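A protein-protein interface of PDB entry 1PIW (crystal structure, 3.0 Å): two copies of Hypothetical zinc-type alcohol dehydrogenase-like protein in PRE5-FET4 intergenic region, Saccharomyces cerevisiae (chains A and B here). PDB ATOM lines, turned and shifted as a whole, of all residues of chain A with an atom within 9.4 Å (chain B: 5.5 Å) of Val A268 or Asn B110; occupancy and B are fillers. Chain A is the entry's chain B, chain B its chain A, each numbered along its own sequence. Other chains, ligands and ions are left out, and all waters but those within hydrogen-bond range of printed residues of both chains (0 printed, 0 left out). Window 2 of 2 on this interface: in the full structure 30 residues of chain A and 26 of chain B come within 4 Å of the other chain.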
ATOM      1  N   LYS A 181       2.930   6.154 -20.133  1.00  0.00           N
ATOM      2  CA  LYS A 181       3.955   5.646 -19.224  1.00  0.00           C
ATOM      3  C   LYS A 181       3.606   4.353 -18.482  1.00  0.00           C
ATOM      4  O   LYS A 181       2.475   4.151 -18.080  1.00  0.00           O
ATOM      5  CB  LYS A 181       4.318   6.745 -18.217  1.00  0.00           C
ATOM      6  CG  LYS A 181       5.005   7.970 -18.845  1.00  0.00           C
ATOM      7  CD  LYS A 181       6.289   7.575 -19.592  1.00  0.00           C
ATOM      8  CE  LYS A 181       6.982   8.763 -20.254  1.00  0.00           C
ATOM      9  NZ  LYS A 181       7.587   9.698 -19.261  1.00  0.00           N
ATOM     10  N   PHE A 241      11.880  -7.577 -19.963  1.00  0.00           N
ATOM     11  CA  PHE A 241      12.937  -6.739 -20.501  1.00  0.00           C
ATOM     12  C   PHE A 241      12.400  -5.542 -21.284  1.00  0.00           C
ATOM     13  O   PHE A 241      11.522  -5.690 -22.133  1.00  0.00           O
ATOM     14  CB  PHE A 241      13.822  -7.586 -21.412  1.00  0.00           C
ATOM     15  CG  PHE A 241      14.767  -6.787 -22.264  1.00  0.00           C
ATOM     16  CD1 PHE A 241      16.049  -6.487 -21.815  1.00  0.00           C
ATOM     17  CD2 PHE A 241      14.375  -6.338 -23.524  1.00  0.00           C
ATOM     18  CE1 PHE A 241      16.933  -5.752 -22.611  1.00  0.00           C
ATOM     19  CE2 PHE A 241      15.245  -5.604 -24.331  1.00  0.00           C
ATOM     20  CZ  PHE A 241      16.528  -5.309 -23.874  1.00  0.00           C
ATOM     21  N   ASP A 242      12.927  -4.359 -20.979  1.00  0.00           N
ATOM     22  CA  ASP A 242      12.575  -3.118 -21.680  1.00  0.00           C
ATOM     23  C   ASP A 242      11.123  -2.662 -21.605  1.00  0.00           C
ATOM     24  O   ASP A 242      10.512  -2.354 -22.631  1.00  0.00           O
ATOM     25  CB  ASP A 242      12.987  -3.247 -23.151  1.00  0.00           C
ATOM     26  CG  ASP A 242      12.841  -1.954 -23.915  1.00  0.00           C
ATOM     27  OD1 ASP A 242      13.441  -0.937 -23.493  1.00  0.00           O
ATOM     28  OD2 ASP A 242      12.132  -1.960 -24.942  1.00  0.00           O
ATOM     29  N   THR A 243      10.583  -2.568 -20.395  1.00  0.00           N
ATOM     30  CA  THR A 243       9.188  -2.168 -20.240  1.00  0.00           C
ATOM     31  C   THR A 243       8.866  -0.919 -19.418  1.00  0.00           C
ATOM     32  O   THR A 243       8.112  -0.050 -19.865  1.00  0.00           O
ATOM     33  CB  THR A 243       8.362  -3.331 -19.654  1.00  0.00           C
ATOM     34  OG1 THR A 243       7.080  -2.840 -19.233  1.00  0.00           O
ATOM     35  CG2 THR A 243       9.088  -3.952 -18.472  1.00  0.00           C
ATOM     36  N   PHE A 244       9.430  -0.841 -18.218  1.00  0.00           N
ATOM     37  CA  PHE A 244       9.170   0.266 -17.305  1.00  0.00           C
ATOM     38  C   PHE A 244       9.893   1.576 -17.559  1.00  0.00           C
ATOM     39  O   PHE A 244      11.090   1.598 -17.838  1.00  0.00           O
ATOM     40  CB  PHE A 244       9.488  -0.171 -15.885  1.00  0.00           C
ATOM     41  CG  PHE A 244       8.720  -1.369 -15.443  1.00  0.00           C
ATOM     42  CD1 PHE A 244       7.375  -1.261 -15.109  1.00  0.00           C
ATOM     43  CD2 PHE A 244       9.340  -2.609 -15.354  1.00  0.00           C
ATOM     44  CE1 PHE A 244       6.660  -2.377 -14.689  1.00  0.00           C
ATOM     45  CE2 PHE A 244       8.635  -3.728 -14.937  1.00  0.00           C
ATOM     46  CZ  PHE A 244       7.292  -3.615 -14.602  1.00  0.00           C
ATOM     47  N   ASP A 245       9.158   2.674 -17.440  1.00  0.00           N
ATOM     48  CA  ASP A 245       9.752   3.987 -17.598  1.00  0.00           C
ATOM     49  C   ASP A 245      10.163   4.356 -16.188  1.00  0.00           C
ATOM     50  O   ASP A 245      11.229   4.922 -15.964  1.00  0.00           O
ATOM     51  CB  ASP A 245       8.725   4.992 -18.104  1.00  0.00           C
ATOM     52  CG  ASP A 245       8.027   4.525 -19.355  1.00  0.00           C
ATOM     53  OD1 ASP A 245       7.976   5.300 -20.340  1.00  0.00           O
ATOM     54  OD2 ASP A 245       7.526   3.380 -19.347  1.00  0.00           O
ATOM     55  N   LEU A 246       9.305   4.002 -15.234  1.00  0.00           N
ATOM     56  CA  LEU A 246       9.548   4.292 -13.831  1.00  0.00           C
ATOM     57  C   LEU A 246       9.252   3.123 -12.905  1.00  0.00           C
ATOM     58  O   LEU A 246       8.389   2.298 -13.186  1.00  0.00           O
ATOM     59  CB  LEU A 246       8.697   5.484 -13.406  1.00  0.00           C
ATOM     60  CG  LEU A 246       8.630   5.837 -11.917  1.00  0.00           C
ATOM     61  CD1 LEU A 246      10.032   6.092 -11.377  1.00  0.00           C
ATOM     62  CD2 LEU A 246       7.741   7.070 -11.720  1.00  0.00           C
ATOM     63  N   PRO A 263      17.227  -3.607 -13.219  1.00  0.00           N
ATOM     64  CA  PRO A 263      17.529  -2.695 -14.325  1.00  0.00           C
ATOM     65  C   PRO A 263      17.099  -3.265 -15.667  1.00  0.00           C
ATOM     66  O   PRO A 263      16.490  -2.580 -16.488  1.00  0.00           O
ATOM     67  CB  PRO A 263      19.041  -2.535 -14.231  1.00  0.00           C
ATOM     68  CG  PRO A 263      19.303  -2.679 -12.776  1.00  0.00           C
ATOM     69  CD  PRO A 263      18.436  -3.860 -12.415  1.00  0.00           C
ATOM     70  N   LYS A 264      17.414  -4.533 -15.872  1.00  0.00           N
ATOM     71  CA  LYS A 264      17.091  -5.194 -17.117  1.00  0.00           C
ATOM     72  C   LYS A 264      15.677  -4.861 -17.592  1.00  0.00           C
ATOM     73  O   LYS A 264      15.459  -4.637 -18.781  1.00  0.00           O
ATOM     74  CB  LYS A 264      17.269  -6.706 -16.946  1.00  0.00           C
ATOM     75  CG  LYS A 264      17.589  -7.455 -18.239  1.00  0.00           C
ATOM     76  CD  LYS A 264      17.925  -8.940 -17.985  1.00  0.00           C
ATOM     77  CE  LYS A 264      19.243  -9.120 -17.239  1.00  0.00           C
ATOM     78  NZ  LYS A 264      19.262  -8.365 -15.947  1.00  0.00           N
ATOM     79  N   ALA A 265      14.729  -4.799 -16.660  1.00  0.00           N
ATOM     80  CA  ALA A 265      13.330  -4.523 -16.991  1.00  0.00           C
ATOM     81  C   ALA A 265      13.020  -3.061 -17.284  1.00  0.00           C
ATOM     82  O   ALA A 265      11.891  -2.722 -17.649  1.00  0.00           O
ATOM     83  CB  ALA A 265      12.426  -5.013 -15.870  1.00  0.00           C
ATOM     84  N   MET A 266      14.015  -2.198 -17.123  1.00  0.00           N
ATOM     85  CA  MET A 266      13.841  -0.773 -17.363  1.00  0.00           C
ATOM     86  C   MET A 266      14.108  -0.422 -18.821  1.00  0.00           C
ATOM     87  O   MET A 266      15.120  -0.826 -19.388  1.00  0.00           O
ATOM     88  CB  MET A 266      14.808   0.016 -16.479  1.00  0.00           C
ATOM     89  CG  MET A 266      14.660  -0.247 -14.997  1.00  0.00           C
ATOM     90  SD  MET A 266      13.004   0.174 -14.496  1.00  0.00           S
ATOM     91  CE  MET A 266      12.906   1.912 -14.937  1.00  0.00           C
ATOM     92  N   LYS A 267      13.209   0.331 -19.434  1.00  0.00           N
ATOM     93  CA  LYS A 267      13.420   0.726 -20.818  1.00  0.00           C
ATOM     94  C   LYS A 267      14.531   1.778 -20.814  1.00  0.00           C
ATOM     95  O   LYS A 267      14.707   2.472 -19.818  1.00  0.00           O
ATOM     96  CB  LYS A 267      12.128   1.296 -21.415  1.00  0.00           C
ATOM     97  CG  LYS A 267      11.413   2.301 -20.534  1.00  0.00           C
ATOM     98  CD  LYS A 267      10.296   3.043 -21.280  1.00  0.00           C
ATOM     99  CE  LYS A 267       9.148   2.135 -21.709  1.00  0.00           C
ATOM    100  NZ  LYS A 267       9.522   1.152 -22.775  1.00  0.00           N
ATOM    101  N   VAL A 268      15.296   1.880 -21.901  1.00  0.00           N
ATOM    102  CA  VAL A 268      16.373   2.868 -21.971  1.00  0.00           C
ATOM    103  C   VAL A 268      15.814   4.205 -21.532  1.00  0.00           C
ATOM    104  O   VAL A 268      14.901   4.729 -22.169  1.00  0.00           O
ATOM    105  CB  VAL A 268      16.913   3.025 -23.410  1.00  0.00           C
ATOM    106  CG1 VAL A 268      17.802   4.264 -23.513  1.00  0.00           C
ATOM    107  CG2 VAL A 268      17.696   1.781 -23.809  1.00  0.00           C
ATOM    108  N   GLY A 269      16.363   4.749 -20.451  1.00  0.00           N
ATOM    109  CA  GLY A 269      15.890   6.017 -19.938  1.00  0.00           C
ATOM    110  C   GLY A 269      15.143   5.800 -18.638  1.00  0.00           C
ATOM    111  O   GLY A 269      14.805   6.745 -17.918  1.00  0.00           O
ATOM    112  N   GLY A 270      14.909   4.530 -18.331  1.00  0.00           N
ATOM    113  CA  GLY A 270      14.179   4.156 -17.131  1.00  0.00           C
ATOM    114  C   GLY A 270      14.720   4.674 -15.816  1.00  0.00           C
ATOM    115  O   GLY A 270      15.929   4.863 -15.659  1.00  0.00           O
ATOM    116  N   ARG A 271      13.819   4.889 -14.860  1.00  0.00           N
ATOM    117  CA  ARG A 271      14.214   5.374 -13.546  1.00  0.00           C
ATOM    118  C   ARG A 271      13.763   4.479 -12.390  1.00  0.00           C
ATOM    119  O   ARG A 271      12.576   4.180 -12.246  1.00  0.00           O
ATOM    120  CB  ARG A 271      13.671   6.779 -13.324  1.00  0.00           C
ATOM    121  CG  ARG A 271      13.942   7.711 -14.472  1.00  0.00           C
ATOM    122  CD  ARG A 271      13.625   9.146 -14.108  1.00  0.00           C
ATOM    123  NE  ARG A 271      13.571   9.989 -15.299  1.00  0.00           N
ATOM    124  CZ  ARG A 271      13.374  11.305 -15.285  1.00  0.00           C
ATOM    125  NH1 ARG A 271      13.215  11.950 -14.135  1.00  0.00           N
ATOM    126  NH2 ARG A 271      13.323  11.978 -16.428  1.00  0.00           N
ATOM    127  N   LEU A 291      24.067   0.188 -14.460  1.00  0.00           N
ATOM    128  CA  LEU A 291      22.911   1.051 -14.679  1.00  0.00           C
ATOM    129  C   LEU A 291      22.984   1.589 -16.107  1.00  0.00           C
ATOM    130  O   LEU A 291      22.945   2.793 -16.327  1.00  0.00           O
ATOM    131  CB  LEU A 291      22.950   2.216 -13.691  1.00  0.00           C
ATOM    132  CG  LEU A 291      23.264   1.826 -12.248  1.00  0.00           C
ATOM    133  CD1 LEU A 291      23.631   3.045 -11.430  1.00  0.00           C
ATOM    134  CD2 LEU A 291      22.067   1.132 -11.654  1.00  0.00           C
ATOM    135  N   LYS A 292      23.098   0.694 -17.079  1.00  0.00           N
ATOM    136  CA  LYS A 292      23.192   1.114 -18.468  1.00  0.00           C
ATOM    137  C   LYS A 292      21.887   1.747 -18.921  1.00  0.00           C
ATOM    138  O   LYS A 292      20.895   1.059 -19.139  1.00  0.00           O
ATOM    139  CB  LYS A 292      23.529  -0.075 -19.367  1.00  0.00           C
ATOM    140  CG  LYS A 292      23.939   0.346 -20.766  1.00  0.00           C
ATOM    141  CD  LYS A 292      24.302  -0.821 -21.683  1.00  0.00           C
ATOM    142  CE  LYS A 292      25.605  -1.496 -21.293  1.00  0.00           C
ATOM    143  NZ  LYS A 292      26.151  -2.210 -22.474  1.00  0.00           N
ATOM    144  N   ALA A 293      21.902   3.071 -19.048  1.00  0.00           N
ATOM    145  CA  ALA A 293      20.742   3.834 -19.476  1.00  0.00           C
ATOM    146  C   ALA A 293      19.645   3.832 -18.424  1.00  0.00           C
ATOM    147  O   ALA A 293      18.486   4.111 -18.725  1.00  0.00           O
ATOM    148  CB  ALA A 293      20.217   3.289 -20.777  1.00  0.00           C
ATOM    149  N   VAL A 294      20.016   3.520 -17.187  1.00  0.00           N
ATOM    150  CA  VAL A 294      19.073   3.517 -16.073  1.00  0.00           C
ATOM    151  C   VAL A 294      19.624   4.339 -14.906  1.00  0.00           C
ATOM    152  O   VAL A 294      20.768   4.146 -14.487  1.00  0.00           O
ATOM    153  CB  VAL A 294      18.809   2.090 -15.583  1.00  0.00           C
ATOM    154  CG1 VAL A 294      18.017   2.110 -14.284  1.00  0.00           C
ATOM    155  CG2 VAL A 294      18.060   1.333 -16.639  1.00  0.00           C
ATOM    156  N   SER A 295      18.822   5.261 -14.384  1.00  0.00           N
ATOM    157  CA  SER A 295      19.280   6.069 -13.259  1.00  0.00           C
ATOM    158  C   SER A 295      18.781   5.408 -11.992  1.00  0.00           C
ATOM    159  O   SER A 295      17.950   4.503 -12.045  1.00  0.00           O
ATOM    160  CB  SER A 295      18.721   7.489 -13.323  1.00  0.00           C
ATOM    161  OG  SER A 295      17.346   7.498 -12.993  1.00  0.00           O
ATOM    162  N   ARG B 105      14.211  -0.312 -29.384  1.00  0.00           N
ATOM    163  CA  ARG B 105      15.383   0.478 -29.052  1.00  0.00           C
ATOM    164  C   ARG B 105      16.091   1.000 -30.294  1.00  0.00           C
ATOM    165  O   ARG B 105      16.525   2.147 -30.333  1.00  0.00           O
ATOM    166  CB  ARG B 105      16.332  -0.349 -28.197  1.00  0.00           C
ATOM    167  CG  ARG B 105      15.741  -0.677 -26.849  1.00  0.00           C
ATOM    168  CD  ARG B 105      16.693  -1.450 -25.959  1.00  0.00           C
ATOM    169  NE  ARG B 105      16.228  -1.431 -24.578  1.00  0.00           N
ATOM    170  CZ  ARG B 105      16.912  -1.930 -23.559  1.00  0.00           C
ATOM    171  NH1 ARG B 105      18.094  -2.489 -23.782  1.00  0.00           N
ATOM    172  NH2 ARG B 105      16.424  -1.865 -22.321  1.00  0.00           N
ATOM    173  N   CYS B 106      16.200   0.172 -31.320  1.00  0.00           N
ATOM    174  CA  CYS B 106      16.844   0.617 -32.546  1.00  0.00           C
ATOM    175  C   CYS B 106      16.034   1.695 -33.266  1.00  0.00           C
ATOM    176  O   CYS B 106      16.553   2.752 -33.612  1.00  0.00           O
ATOM    177  CB  CYS B 106      17.039  -0.559 -33.494  1.00  0.00           C
ATOM    178  SG  CYS B 106      18.471  -1.537 -33.137  1.00  0.00           S
ATOM    179  N   ASN B 108      13.927   3.526 -32.132  1.00  0.00           N
ATOM    180  CA  ASN B 108      13.738   4.676 -31.280  1.00  0.00           C
ATOM    181  C   ASN B 108      15.075   5.389 -30.998  1.00  0.00           C
ATOM    182  O   ASN B 108      15.198   6.165 -30.051  1.00  0.00           O
ATOM    183  CB  ASN B 108      13.058   4.227 -29.990  1.00  0.00           C
ATOM    184  CG  ASN B 108      12.030   5.224 -29.510  1.00  0.00           C
ATOM    185  OD1 ASN B 108      12.360   6.215 -28.834  1.00  0.00           O
ATOM    186  ND2 ASN B 108      10.769   4.984 -29.876  1.00  0.00           N
ATOM    187  N   ASP B 109      16.067   5.114 -31.837  1.00  0.00           N
ATOM    188  CA  ASP B 109      17.387   5.725 -31.728  1.00  0.00           C
ATOM    189  C   ASP B 109      18.111   5.433 -30.428  1.00  0.00           C
ATOM    190  O   ASP B 109      18.538   6.334 -29.710  1.00  0.00           O
ATOM    191  CB  ASP B 109      17.277   7.231 -31.937  1.00  0.00           C
ATOM    192  CG  ASP B 109      16.644   7.582 -33.268  1.00  0.00           C
ATOM    193  OD1 ASP B 109      17.214   7.190 -34.316  1.00  0.00           O
ATOM    194  OD2 ASP B 109      15.578   8.243 -33.261  1.00  0.00           O
ATOM    195  N   ASN B 110      18.246   4.147 -30.140  1.00  0.00           N
ATOM    196  CA  ASN B 110      18.942   3.686 -28.948  1.00  0.00           C
ATOM    197  C   ASN B 110      19.718   2.422 -29.273  1.00  0.00           C
ATOM    198  O   ASN B 110      19.849   1.526 -28.449  1.00  0.00           O
ATOM    199  CB  ASN B 110      17.950   3.438 -27.808  1.00  0.00           C
ATOM    200  CG  ASN B 110      17.499   4.730 -27.145  1.00  0.00           C
ATOM    201  OD1 ASN B 110      18.321   5.537 -26.710  1.00  0.00           O
ATOM    202  ND2 ASN B 110      16.193   4.929 -27.064  1.00  0.00           N
ATOM    203  N   GLU B 111      20.258   2.383 -30.487  1.00  0.00           N
ATOM    204  CA  GLU B 111      21.016   1.243 -30.942  1.00  0.00           C
ATOM    205  C   GLU B 111      22.232   0.947 -30.094  1.00  0.00           C
ATOM    206  O   GLU B 111      22.793  -0.137 -30.180  1.00  0.00           O
ATOM    207  CB  GLU B 111      21.425   1.417 -32.398  1.00  0.00           C
ATOM    208  CG  GLU B 111      22.053   2.747 -32.732  1.00  0.00           C
ATOM    209  CD  GLU B 111      21.048   3.744 -33.251  1.00  0.00           C
ATOM    210  OE1 GLU B 111      20.388   4.400 -32.422  1.00  0.00           O
ATOM    211  OE2 GLU B 111      20.915   3.859 -34.488  1.00  0.00           O
ATOM    212  N   PRO B 112      22.689   1.911 -29.286  1.00  0.00           N
ATOM    213  CA  PRO B 112      23.859   1.556 -28.479  1.00  0.00           C
ATOM    214  C   PRO B 112      23.428   0.554 -27.420  1.00  0.00           C
ATOM    215  O   PRO B 112      24.247  -0.166 -26.867  1.00  0.00           O
ATOM    216  CB  PRO B 112      24.262   2.884 -27.856  1.00  0.00           C
ATOM    217  CG  PRO B 112      23.868   3.871 -28.892  1.00  0.00           C
ATOM    218  CD  PRO B 112      22.507   3.371 -29.315  1.00  0.00           C
ATOM    219  N   TYR B 113      22.126   0.515 -27.156  1.00  0.00           N
ATOM    220  CA  TYR B 113      21.550  -0.375 -26.155  1.00  0.00           C
ATOM    221  C   TYR B 113      20.778  -1.531 -26.784  1.00  0.00           C
ATOM    222  O   TYR B 113      19.899  -2.126 -26.150  1.00  0.00           O
ATOM    223  CB  TYR B 113      20.622   0.424 -25.234  1.00  0.00           C
ATOM    224  CG  TYR B 113      21.260   1.688 -24.733  1.00  0.00           C
ATOM    225  CD1 TYR B 113      21.360   2.809 -25.548  1.00  0.00           C
ATOM    226  CD2 TYR B 113      21.863   1.733 -23.483  1.00  0.00           C
ATOM    227  CE1 TYR B 113      22.062   3.944 -25.126  1.00  0.00           C
ATOM    228  CE2 TYR B 113      22.564   2.852 -23.052  1.00  0.00           C
ATOM    229  CZ  TYR B 113      22.663   3.950 -23.873  1.00  0.00           C
ATOM    230  OH  TYR B 113      23.370   5.048 -23.453  1.00  0.00           O
ATOM    231  N   CYS B 114      21.090  -1.844 -28.037  1.00  0.00           N
ATOM    232  CA  CYS B 114      20.418  -2.943 -28.710  1.00  0.00           C
ATOM    233  C   CYS B 114      20.972  -4.256 -28.200  1.00  0.00           C
ATOM    234  O   CYS B 114      22.135  -4.350 -27.828  1.00  0.00           O
ATOM    235  CB  CYS B 114      20.615  -2.864 -30.224  1.00  0.00           C
ATOM    236  SG  CYS B 114      20.162  -4.388 -31.093  1.00  0.00           S
ATOM    237  N   ARG B 174      20.719  14.362 -23.885  1.00  0.00           N
ATOM    238  CA  ARG B 174      19.711  13.639 -23.148  1.00  0.00           C
ATOM    239  C   ARG B 174      19.443  14.201 -21.752  1.00  0.00           C
ATOM    240  O   ARG B 174      18.313  14.189 -21.294  1.00  0.00           O
ATOM    241  CB  ARG B 174      20.117  12.170 -23.050  1.00  0.00           C
ATOM    242  CG  ARG B 174      20.367  11.539 -24.404  1.00  0.00           C
ATOM    243  CD  ARG B 174      20.372  10.024 -24.340  1.00  0.00           C
ATOM    244  NE  ARG B 174      20.434   9.444 -25.676  1.00  0.00           N
ATOM    245  CZ  ARG B 174      20.002   8.230 -25.972  1.00  0.00           C
ATOM    246  NH1 ARG B 174      19.475   7.481 -25.012  1.00  0.00           N
ATOM    247  NH2 ARG B 174      20.097   7.767 -27.212  1.00  0.00           N
ATOM    248  N   SER B 303      23.669   7.584 -30.102  1.00  0.00           N
ATOM    249  CA  SER B 303      22.941   7.047 -31.238  1.00  0.00           C
ATOM    250  C   SER B 303      23.601   7.682 -32.451  1.00  0.00           C
ATOM    251  O   SER B 303      24.302   8.690 -32.329  1.00  0.00           O
ATOM    252  CB  SER B 303      21.491   7.492 -31.184  1.00  0.00           C
ATOM    253  OG  SER B 303      21.419   8.906 -31.275  1.00  0.00           O
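No position is printed for both chains. Of the 9 pairs that touch across the chains among the printed residues, none has its exchanged pair printed and touching as well.
Thr A243 touches none of the printed residues of chain B. Val A268 touches just these residues of chain B: Arg B105 (3.6 Å), Asn B110 (3.5 Å), Tyr B113 (3.5 Å) and Arg B174 (3.9 Å). Leu A291 touches none of the printed residues of chain B. Of the printed residues of chain B, Lys A292 touches Tyr B113. Glu B111 touches none of the printed residues of chain A. Printed residues of chain A within 4 Å of Tyr B113: Val A268, Lys A292 and Ala A293. The nearest printed residue of chain A that does not touch Tyr B113 is Phe A241 (5.2 Å).
Of the 11 printed residues of chain B, 4 touch a printed residue of chain A. Printed residues of chain B that touch a printed residue of chain A: Arg B105, Asn B110, Tyr B113 and Arg B174.
The guanidinium group (NH2) of Arg B105 sits at hydrogen-bond distance from the backbone carbonyl oxygen (O) of Met A266. OD1 of Asp A242 is in salt-bridge range of NE of Arg B105 (3.0 Å).
N of Asp A242 sits at hydrogen-bond distance from O of Lys A264, at 3.4 Å. N of Asn B110 lies within hydrogen-bond range of O of Arg B105, at 2.6 Å. The backbone carbonyl oxygen (O) of Tyr B113 is in hydrogen-bond range of the guanidinium group (NH1) of Arg B105 (3.0 Å). N of Gly A269 lies within hydrogen-bond range of O of Ala A293. The side-chain amide nitrogen (ND2) of Asn B110 is in hydrogen-bond range of the backbone carbonyl oxygen (O) of Asn B108 (3.4 Å). The backbone carbonyl oxygen of Asp B109 sits at hydrogen-bond distance from the guanidinium group of Arg B174, at 3.3 Å.
Arg B105 touches Phe A241 (NH1 to CZ, 3.2 Å). Val A268 touches Arg B105 (CG2 to NE, 3.6 Å). Val A268 touches Asn B110 (CG1 to OD1, 3.5 Å). CG2 of Val A268 touches CB of Tyr B113, at 3.5 Å. CG1 of Val A268 touches NH1 of Arg B174, at 3.9 Å. CG of Lys A292 touches CE2 of Tyr B113 (3.7 Å). Ala A293 touches Tyr B113 (CB to CE2, 3.3 Å).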
